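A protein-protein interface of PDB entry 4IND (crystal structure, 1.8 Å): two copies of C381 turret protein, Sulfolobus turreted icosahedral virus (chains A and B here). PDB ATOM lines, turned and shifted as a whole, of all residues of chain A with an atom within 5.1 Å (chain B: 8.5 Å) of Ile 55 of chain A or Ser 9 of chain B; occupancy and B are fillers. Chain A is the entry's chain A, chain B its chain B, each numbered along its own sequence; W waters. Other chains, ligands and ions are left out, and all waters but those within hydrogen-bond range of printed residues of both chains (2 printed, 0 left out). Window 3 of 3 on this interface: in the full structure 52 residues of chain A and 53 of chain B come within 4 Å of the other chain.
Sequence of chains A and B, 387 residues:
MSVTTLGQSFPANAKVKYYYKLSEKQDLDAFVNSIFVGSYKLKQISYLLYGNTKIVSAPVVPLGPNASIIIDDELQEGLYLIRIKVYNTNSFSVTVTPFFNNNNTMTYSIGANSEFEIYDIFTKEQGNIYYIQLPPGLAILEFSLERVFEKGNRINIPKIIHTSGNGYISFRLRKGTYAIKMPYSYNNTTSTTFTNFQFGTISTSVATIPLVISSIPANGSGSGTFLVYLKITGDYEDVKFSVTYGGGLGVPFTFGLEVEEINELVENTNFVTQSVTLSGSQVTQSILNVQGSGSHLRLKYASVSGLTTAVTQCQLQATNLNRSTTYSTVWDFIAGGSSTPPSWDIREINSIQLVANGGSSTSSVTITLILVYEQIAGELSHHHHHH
The backbone carbonyl oxygen of Pro 11 of chain B is in hydrogen-bond range of the backbone NH of Ser 34 of chain B, at 3.4 Å. The backbone NH (N) of Ile 45 of chain A sits at hydrogen-bond distance from the backbone carbonyl oxygen (O) of Val 56 of chain A, 2.7 Å away. N of Asn 13 of chain B sits at hydrogen-bond distance from O of Asn 33 of chain B (3.1 Å).
Water W1 lies within hydrogen-bond range of O of Ser 34 of chain B (2.7 Å) and NZ of Lys 54 of chain A (3.0 Å). Water W2 bridges the backbone carbonyl oxygen of Ile 55 of chain A and the side-chain amide nitrogen of Asn 13 of chain B.
No position is printed for both chains. Of the 12 pairs that touch across the chains among the printed residues, none has its exchanged pair printed and touching as well.
The backbone carbonyl oxygen (O) of Thr 53 of chain A lies within hydrogen-bond range of the backbone NH (N) of Phe 10 of chain B (2.7 Å). N of Thr 53 of chain A lies within hydrogen-bond range of O of Gln 8 of chain B, at 2.7 Å. N of Ala 12 of chain B is in hydrogen-bond range of O of Ile 55 of chain A, at 2.9 Å. The backbone NH (N) of Ser 57 of chain A lies within hydrogen-bond range of the side-chain amide oxygen (OD1) of Asn 13 of chain B, at 2.8 Å. N of Ile 55 of chain A lies within hydrogen-bond range of O of Phe 10 of chain B.
Among the printed residues, 12 pairs touch across the chains.
Ile 55 of chain A touches just these residues of chain B: Ser 9, Phe 10, Pro 11 and Ala 12. Of the printed residues of chain A, Ser 9 of chain B touches Thr 53 (3.0 Å) and Ile 55 (3.7 Å). Of the printed residues of chain B, Val 56 of chain A touches Ala 12 and Asn 13. Of the printed residues of chain B, Ser 57 of chain A touches Asn 13 (2.8 Å). Of the printed residues of chain A, Pro 11 of chain B touches Ile 55 (3.4 Å). Printed residues of chain A within 4 Å of Phe 10 of chain B: Thr 53, Lys 54 and Ile 55. Of the printed residues of chain B, Lys 54 of chain A touches Phe 10 and Ala 12. Gly 7 of chain B touches none of the printed residues of chain A. Ala 14 of chain B touches none of the printed residues of chain A. The nearest printed residue of chain A that does not touch Pro 11 of chain B is Val 56 of chain A (5.3 Å).
O of Thr 53 of chain A touches CA of Ser 9 of chain B (3.0 Å). Phe 10 of chain B touches Lys 54 of chain A. CG of Lys 54 of chain A touches CB of Ala 12 of chain B, at 3.5 Å. Ser 9 of chain B touches Ile 55 of chain A (CB to CD1, 3.7 Å). O of Ile 55 of chain A touches CA of Pro 11 of chain B, at 3.4 Å. CG1 of Val 56 of chain A touches O of Ala 12 of chain B, at 3.2 Å. Asn 13 of chain B touches Val 56 of chain A (OD1 to CA, 3.2 Å).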
ATOM      1  N   GLN A  44     -15.745   7.245 -13.548  1.00  0.00           N
ATOM      2  CA  GLN A  44     -16.516   6.051 -13.798  1.00  0.00           C
ATOM      3  C   GLN A  44     -15.597   4.969 -14.367  1.00  0.00           C
ATOM      4  O   GLN A  44     -14.948   5.165 -15.400  1.00  0.00           O
ATOM      5  CB  GLN A  44     -17.679   6.342 -14.743  1.00  0.00           C
ATOM      6  CG  GLN A  44     -18.621   5.157 -14.864  1.00  0.00           C
ATOM      7  CD  GLN A  44     -19.993   5.540 -15.363  1.00  0.00           C
ATOM      8  OE1 GLN A  44     -20.856   5.983 -14.595  1.00  0.00           O
ATOM      9  NE2 GLN A  44     -20.210   5.358 -16.659  1.00  0.00           N
ATOM     10  N   ILE A  45     -15.551   3.834 -13.686  1.00  0.00           N
ATOM     11  CA  ILE A  45     -14.636   2.740 -13.989  1.00  0.00           C
ATOM     12  C   ILE A  45     -15.458   1.531 -14.460  1.00  0.00           C
ATOM     13  O   ILE A  45     -16.447   1.160 -13.833  1.00  0.00           O
ATOM     14  CB  ILE A  45     -13.852   2.332 -12.701  1.00  0.00           C
ATOM     15  CG1 ILE A  45     -12.898   3.451 -12.271  1.00  0.00           C
ATOM     16  CG2 ILE A  45     -13.132   0.999 -12.872  1.00  0.00           C
ATOM     17  CD1 ILE A  45     -12.015   3.968 -13.370  1.00  0.00           C
ATOM     18  N   SER A  46     -15.035   0.898 -15.546  1.00  0.00           N
ATOM     19  CA  SER A  46     -15.735  -0.270 -16.057  1.00  0.00           C
ATOM     20  C   SER A  46     -14.750  -1.407 -16.305  1.00  0.00           C
ATOM     21  O   SER A  46     -13.666  -1.191 -16.842  1.00  0.00           O
ATOM     22  CB  SER A  46     -16.412   0.069 -17.390  1.00  0.00           C
ATOM     23  OG  SER A  46     -17.296   1.162 -17.264  1.00  0.00           O
ATOM     24  N   THR A  53     -20.218  -6.155 -17.814  1.00  0.00           N
ATOM     25  CA  THR A  53     -19.446  -4.968 -17.468  1.00  0.00           C
ATOM     26  C   THR A  53     -19.873  -4.380 -16.126  1.00  0.00           C
ATOM     27  O   THR A  53     -20.964  -3.824 -15.987  1.00  0.00           O
ATOM     28  CB  THR A  53     -19.559  -3.906 -18.551  1.00  0.00           C
ATOM     29  OG1 THR A  53     -19.114  -4.453 -19.795  1.00  0.00           O
ATOM     30  CG2 THR A  53     -18.708  -2.714 -18.209  1.00  0.00           C
ATOM     31  N   LYS A  54     -18.996  -4.517 -15.138  1.00  0.00           N
ATOM     32  CA  LYS A  54     -19.229  -3.909 -13.833  1.00  0.00           C
ATOM     33  C   LYS A  54     -18.868  -2.431 -13.936  1.00  0.00           C
ATOM     34  O   LYS A  54     -17.805  -2.082 -14.440  1.00  0.00           O
ATOM     35  CB  LYS A  54     -18.363  -4.589 -12.771  1.00  0.00           C
ATOM     36  CG  LYS A  54     -18.416  -3.930 -11.390  1.00  0.00           C
ATOM     37  CD  LYS A  54     -17.701  -4.785 -10.326  1.00  0.00           C
ATOM     38  CE  LYS A  54     -17.340  -3.945  -9.116  1.00  0.00           C
ATOM     39  NZ  LYS A  54     -17.029  -4.769  -7.901  1.00  0.00           N
ATOM     40  N   ILE A  55     -19.757  -1.561 -13.474  1.00  0.00           N
ATOM     41  CA  ILE A  55     -19.503  -0.132 -13.540  1.00  0.00           C
ATOM     42  C   ILE A  55     -19.571   0.461 -12.126  1.00  0.00           C
ATOM     43  O   ILE A  55     -20.580   0.299 -11.434  1.00  0.00           O
ATOM     44  CB  ILE A  55     -20.525   0.564 -14.436  1.00  0.00           C
ATOM     45  CG1 ILE A  55     -20.504  -0.053 -15.834  1.00  0.00           C
ATOM     46  CG2 ILE A  55     -20.239   2.053 -14.523  1.00  0.00           C
ATOM     47  CD1 ILE A  55     -21.525   0.575 -16.792  1.00  0.00           C
ATOM     48  N   VAL A  56     -18.481   1.101 -11.703  1.00  0.00           N
ATOM     49  CA  VAL A  56     -18.460   1.839 -10.428  1.00  0.00           C
ATOM     50  C   VAL A  56     -17.866   3.252 -10.603  1.00  0.00           C
ATOM     51  O   VAL A  56     -17.157   3.527 -11.577  1.00  0.00           O
ATOM     52  CB  VAL A  56     -17.683   1.090  -9.339  1.00  0.00           C
ATOM     53  CG1 VAL A  56     -18.338  -0.248  -9.029  1.00  0.00           C
ATOM     54  CG2 VAL A  56     -16.229   0.891  -9.764  1.00  0.00           C
ATOM     55  N   SER A  57     -18.169   4.152  -9.676  1.00  0.00           N
ATOM     56  CA  SER A  57     -17.463   5.435  -9.605  1.00  0.00           C
ATOM     57  C   SER A  57     -16.459   5.335  -8.473  1.00  0.00           C
ATOM     58  O   SER A  57     -16.844   5.078  -7.341  1.00  0.00           O
ATOM     59  CB  SER A  57     -18.444   6.568  -9.327  1.00  0.00           C
ATOM     60  OG  SER A  57     -19.332   6.714 -10.406  1.00  0.00           O
ATOM     61  N   LEU B   6     -24.663 -10.893 -25.146  1.00  0.00           N
ATOM     62  CA  LEU B   6     -25.048 -11.683 -23.977  1.00  0.00           C
ATOM     63  C   LEU B   6     -24.644 -11.009 -22.665  1.00  0.00           C
ATOM     64  O   LEU B   6     -25.368 -11.088 -21.669  1.00  0.00           O
ATOM     65  CB  LEU B   6     -24.451 -13.092 -24.057  1.00  0.00           C
ATOM     66  CG  LEU B   6     -25.065 -14.119 -23.102  1.00  0.00           C
ATOM     67  CD1 LEU B   6     -26.572 -14.173 -23.309  1.00  0.00           C
ATOM     68  CD2 LEU B   6     -24.442 -15.503 -23.279  1.00  0.00           C
ATOM     69  N   GLY B   7     -23.486 -10.348 -22.666  1.00  0.00           N
ATOM     70  CA  GLY B   7     -23.023  -9.627 -21.492  1.00  0.00           C
ATOM     71  C   GLY B   7     -23.788  -8.334 -21.306  1.00  0.00           C
ATOM     72  O   GLY B   7     -24.242  -7.736 -22.280  1.00  0.00           O
ATOM     73  N   GLN B   8     -23.928  -7.904 -20.056  1.00  0.00           N
ATOM     74  CA  GLN B   8     -24.614  -6.662 -19.740  1.00  0.00           C
ATOM     75  C   GLN B   8     -23.729  -5.852 -18.818  1.00  0.00           C
ATOM     76  O   GLN B   8     -22.843  -6.408 -18.156  1.00  0.00           O
ATOM     77  CB  GLN B   8     -25.924  -6.949 -18.998  1.00  0.00           C
ATOM     78  CG  GLN B   8     -26.934  -7.762 -19.756  1.00  0.00           C
ATOM     79  CD  GLN B   8     -28.161  -8.045 -18.924  1.00  0.00           C
ATOM     80  OE1 GLN B   8     -29.024  -7.184 -18.758  1.00  0.00           O
ATOM     81  NE2 GLN B   8     -28.244  -9.252 -18.385  1.00  0.00           N
ATOM     82  N   SER B   9     -23.975  -4.548 -18.766  1.00  0.00           N
ATOM     83  CA  SER B   9     -23.326  -3.698 -17.792  1.00  0.00           C
ATOM     84  C   SER B   9     -24.200  -3.689 -16.530  1.00  0.00           C
ATOM     85  O   SER B   9     -25.415  -3.914 -16.606  1.00  0.00           O
ATOM     86  CB  SER B   9     -23.149  -2.294 -18.368  1.00  0.00           C
ATOM     87  OG  SER B   9     -24.397  -1.670 -18.538  1.00  0.00           O
ATOM     88  N   PHE B  10     -23.576  -3.486 -15.374  1.00  0.00           N
ATOM     89  CA  PHE B  10     -24.319  -3.350 -14.133  1.00  0.00           C
ATOM     90  C   PHE B  10     -23.606  -2.401 -13.194  1.00  0.00           C
ATOM     91  O   PHE B  10     -22.373  -2.383 -13.153  1.00  0.00           O
ATOM     92  CB  PHE B  10     -24.563  -4.720 -13.463  1.00  0.00           C
ATOM     93  CG  PHE B  10     -23.313  -5.427 -12.996  1.00  0.00           C
ATOM     94  CD1 PHE B  10     -23.023  -5.534 -11.634  1.00  0.00           C
ATOM     95  CD2 PHE B  10     -22.451  -6.027 -13.904  1.00  0.00           C
ATOM     96  CE1 PHE B  10     -21.887  -6.203 -11.198  1.00  0.00           C
ATOM     97  CE2 PHE B  10     -21.310  -6.705 -13.475  1.00  0.00           C
ATOM     98  CZ  PHE B  10     -21.028  -6.801 -12.123  1.00  0.00           C
ATOM     99  N   PRO B  11     -24.378  -1.616 -12.430  1.00  0.00           N
ATOM    100  CA  PRO B  11     -23.801  -0.712 -11.427  1.00  0.00           C
ATOM    101  C   PRO B  11     -23.397  -1.508 -10.196  1.00  0.00           C
ATOM    102  O   PRO B  11     -24.125  -2.414  -9.787  1.00  0.00           O
ATOM    103  CB  PRO B  11     -24.982   0.225 -11.096  1.00  0.00           C
ATOM    104  CG  PRO B  11     -26.193  -0.649 -11.269  1.00  0.00           C
ATOM    105  CD  PRO B  11     -25.854  -1.566 -12.450  1.00  0.00           C
ATOM    106  N   ALA B  12     -22.246  -1.201  -9.604  1.00  0.00           N
ATOM    107  CA  ALA B  12     -21.794  -2.002  -8.478  1.00  0.00           C
ATOM    108  C   ALA B  12     -21.152  -1.182  -7.379  1.00  0.00           C
ATOM    109  O   ALA B  12     -20.178  -1.623  -6.774  1.00  0.00           O
ATOM    110  CB  ALA B  12     -20.816  -3.106  -8.971  1.00  0.00           C
ATOM    111  N   ASN B  13     -21.707  -0.004  -7.096  1.00  0.00           N
ATOM    112  CA  ASN B  13     -21.083   0.870  -6.118  1.00  0.00           C
ATOM    113  C   ASN B  13     -21.223   0.499  -4.652  1.00  0.00           C
ATOM    114  O   ASN B  13     -20.390   0.909  -3.828  1.00  0.00           O
ATOM    115  CB  ASN B  13     -21.589   2.280  -6.317  1.00  0.00           C
ATOM    116  CG  ASN B  13     -21.316   2.770  -7.710  1.00  0.00           C
ATOM    117  OD1 ASN B  13     -20.167   3.081  -8.057  1.00  0.00           O
ATOM    118  ND2 ASN B  13     -22.360   2.787  -8.547  1.00  0.00           N
ATOM    119  N   ALA B  14     -22.290  -0.220  -4.321  1.00  0.00           N
ATOM    120  CA  ALA B  14     -22.646  -0.426  -2.918  1.00  0.00           C
ATOM    121  C   ALA B  14     -21.867  -1.574  -2.301  1.00  0.00           C
ATOM    122  O   ALA B  14     -21.513  -2.539  -2.990  1.00  0.00           O
ATOM    123  CB  ALA B  14     -24.160  -0.685  -2.767  1.00  0.00           C
ATOM    124  N   VAL B  32     -29.019  -4.670  -6.014  1.00  0.00           N
ATOM    125  CA  VAL B  32     -29.010  -4.268  -7.417  1.00  0.00           C
ATOM    126  C   VAL B  32     -28.064  -3.121  -7.720  1.00  0.00           C
ATOM    127  O   VAL B  32     -28.100  -2.574  -8.810  1.00  0.00           O
ATOM    128  CB  VAL B  32     -30.437  -3.982  -7.964  1.00  0.00           C
ATOM    129  CG1 VAL B  32     -31.350  -5.172  -7.719  1.00  0.00           C
ATOM    130  CG2 VAL B  32     -31.042  -2.704  -7.355  1.00  0.00           C
ATOM    131  N   ASN B  33     -27.220  -2.767  -6.753  1.00  0.00           N
ATOM    132  CA  ASN B  33     -26.160  -1.761  -6.960  1.00  0.00           C
ATOM    133  C   ASN B  33     -24.864  -2.364  -6.459  1.00  0.00           C
ATOM    134  O   ASN B  33     -24.018  -1.677  -5.896  1.00  0.00           O
ATOM    135  CB  ASN B  33     -26.491  -0.433  -6.252  1.00  0.00           C
ATOM    136  CG  ASN B  33     -25.483   0.686  -6.563  1.00  0.00           C
ATOM    137  OD1 ASN B  33     -24.724   0.621  -7.548  1.00  0.00           O
ATOM    138  ND2 ASN B  33     -25.484   1.728  -5.730  1.00  0.00           N
ATOM    139  N   SER B  34     -24.712  -3.682  -6.663  1.00  0.00           N
ATOM    140  CA  SER B  34     -23.501  -4.358  -6.213  1.00  0.00           C
ATOM    141  C   SER B  34     -23.236  -5.685  -6.916  1.00  0.00           C
ATOM    142  O   SER B  34     -22.169  -5.901  -7.507  1.00  0.00           O
ATOM    143  CB  SER B  34     -23.541  -4.570  -4.693  1.00  0.00           C
ATOM    144  OG  SER B  34     -24.654  -5.340  -4.288  1.00  0.00           O
ATOM    145  N   PHE B  36     -26.020  -7.821  -8.471  1.00  0.00           N
ATOM    146  CA  PHE B  36     -27.061  -8.297  -9.382  1.00  0.00           C
ATOM    147  C   PHE B  36     -26.918  -7.709 -10.789  1.00  0.00           C
ATOM    148  O   PHE B  36     -26.770  -6.510 -10.961  1.00  0.00           O
ATOM    149  CB  PHE B  36     -28.460  -8.014  -8.828  1.00  0.00           C
ATOM    150  CG  PHE B  36     -29.579  -8.569  -9.681  1.00  0.00           C
ATOM    151  CD1 PHE B  36     -29.902  -9.918  -9.633  1.00  0.00           C
ATOM    152  CD2 PHE B  36     -30.326  -7.738 -10.513  1.00  0.00           C
ATOM    153  CE1 PHE B  36     -30.954 -10.422 -10.417  1.00  0.00           C
ATOM    154  CE2 PHE B  36     -31.379  -8.236 -11.287  1.00  0.00           C
ATOM    155  CZ  PHE B  36     -31.682  -9.579 -11.241  1.00  0.00           C
ATOM    156  N   VAL B  37     -26.979  -8.571 -11.795  1.00  0.00           N
ATOM    157  CA  VAL B  37     -26.809  -8.167 -13.187  1.00  0.00           C
ATOM    158  C   VAL B  37     -28.119  -8.418 -13.925  1.00  0.00           C
ATOM    159  O   VAL B  37     -28.646  -9.535 -13.910  1.00  0.00           O
ATOM    160  CB  VAL B  37     -25.688  -8.973 -13.866  1.00  0.00           C
ATOM    161  CG1 VAL B  37     -25.454  -8.492 -15.300  1.00  0.00           C
ATOM    162  CG2 VAL B  37     -24.399  -8.883 -13.050  1.00  0.00           C
ATOM    163  N   GLY B  38     -28.639  -7.381 -14.584  1.00  0.00           N
ATOM    164  CA  GLY B  38     -29.875  -7.496 -15.337  1.00  0.00           C
ATOM    165  C   GLY B  38     -31.003  -6.701 -14.705  1.00  0.00           C
ATOM    166  O   GLY B  38     -30.799  -5.987 -13.720  1.00  0.00           O
ATOM    167  N   SER B  39     -32.197  -6.851 -15.272  1.00  0.00           N
ATOM    168  CA  SER B  39     -33.389  -6.185 -14.761  1.00  0.00           C
ATOM    169  C   SER B  39     -34.171  -7.074 -13.804  1.00  0.00           C
ATOM    170  O   SER B  39     -33.938  -8.276 -13.724  1.00  0.00           O
ATOM    171  CB  SER B  39     -34.286  -5.759 -15.925  1.00  0.00           C
ATOM    172  OG  SER B  39     -33.631  -4.807 -16.742  1.00  0.00           O
HETATM  173  O   HOH W   1     -19.661  -5.526  -6.669  1.00  0.00           O
HETATM  174  O   HOH W   2     -22.249   2.579 -11.582  1.00  0.00           O
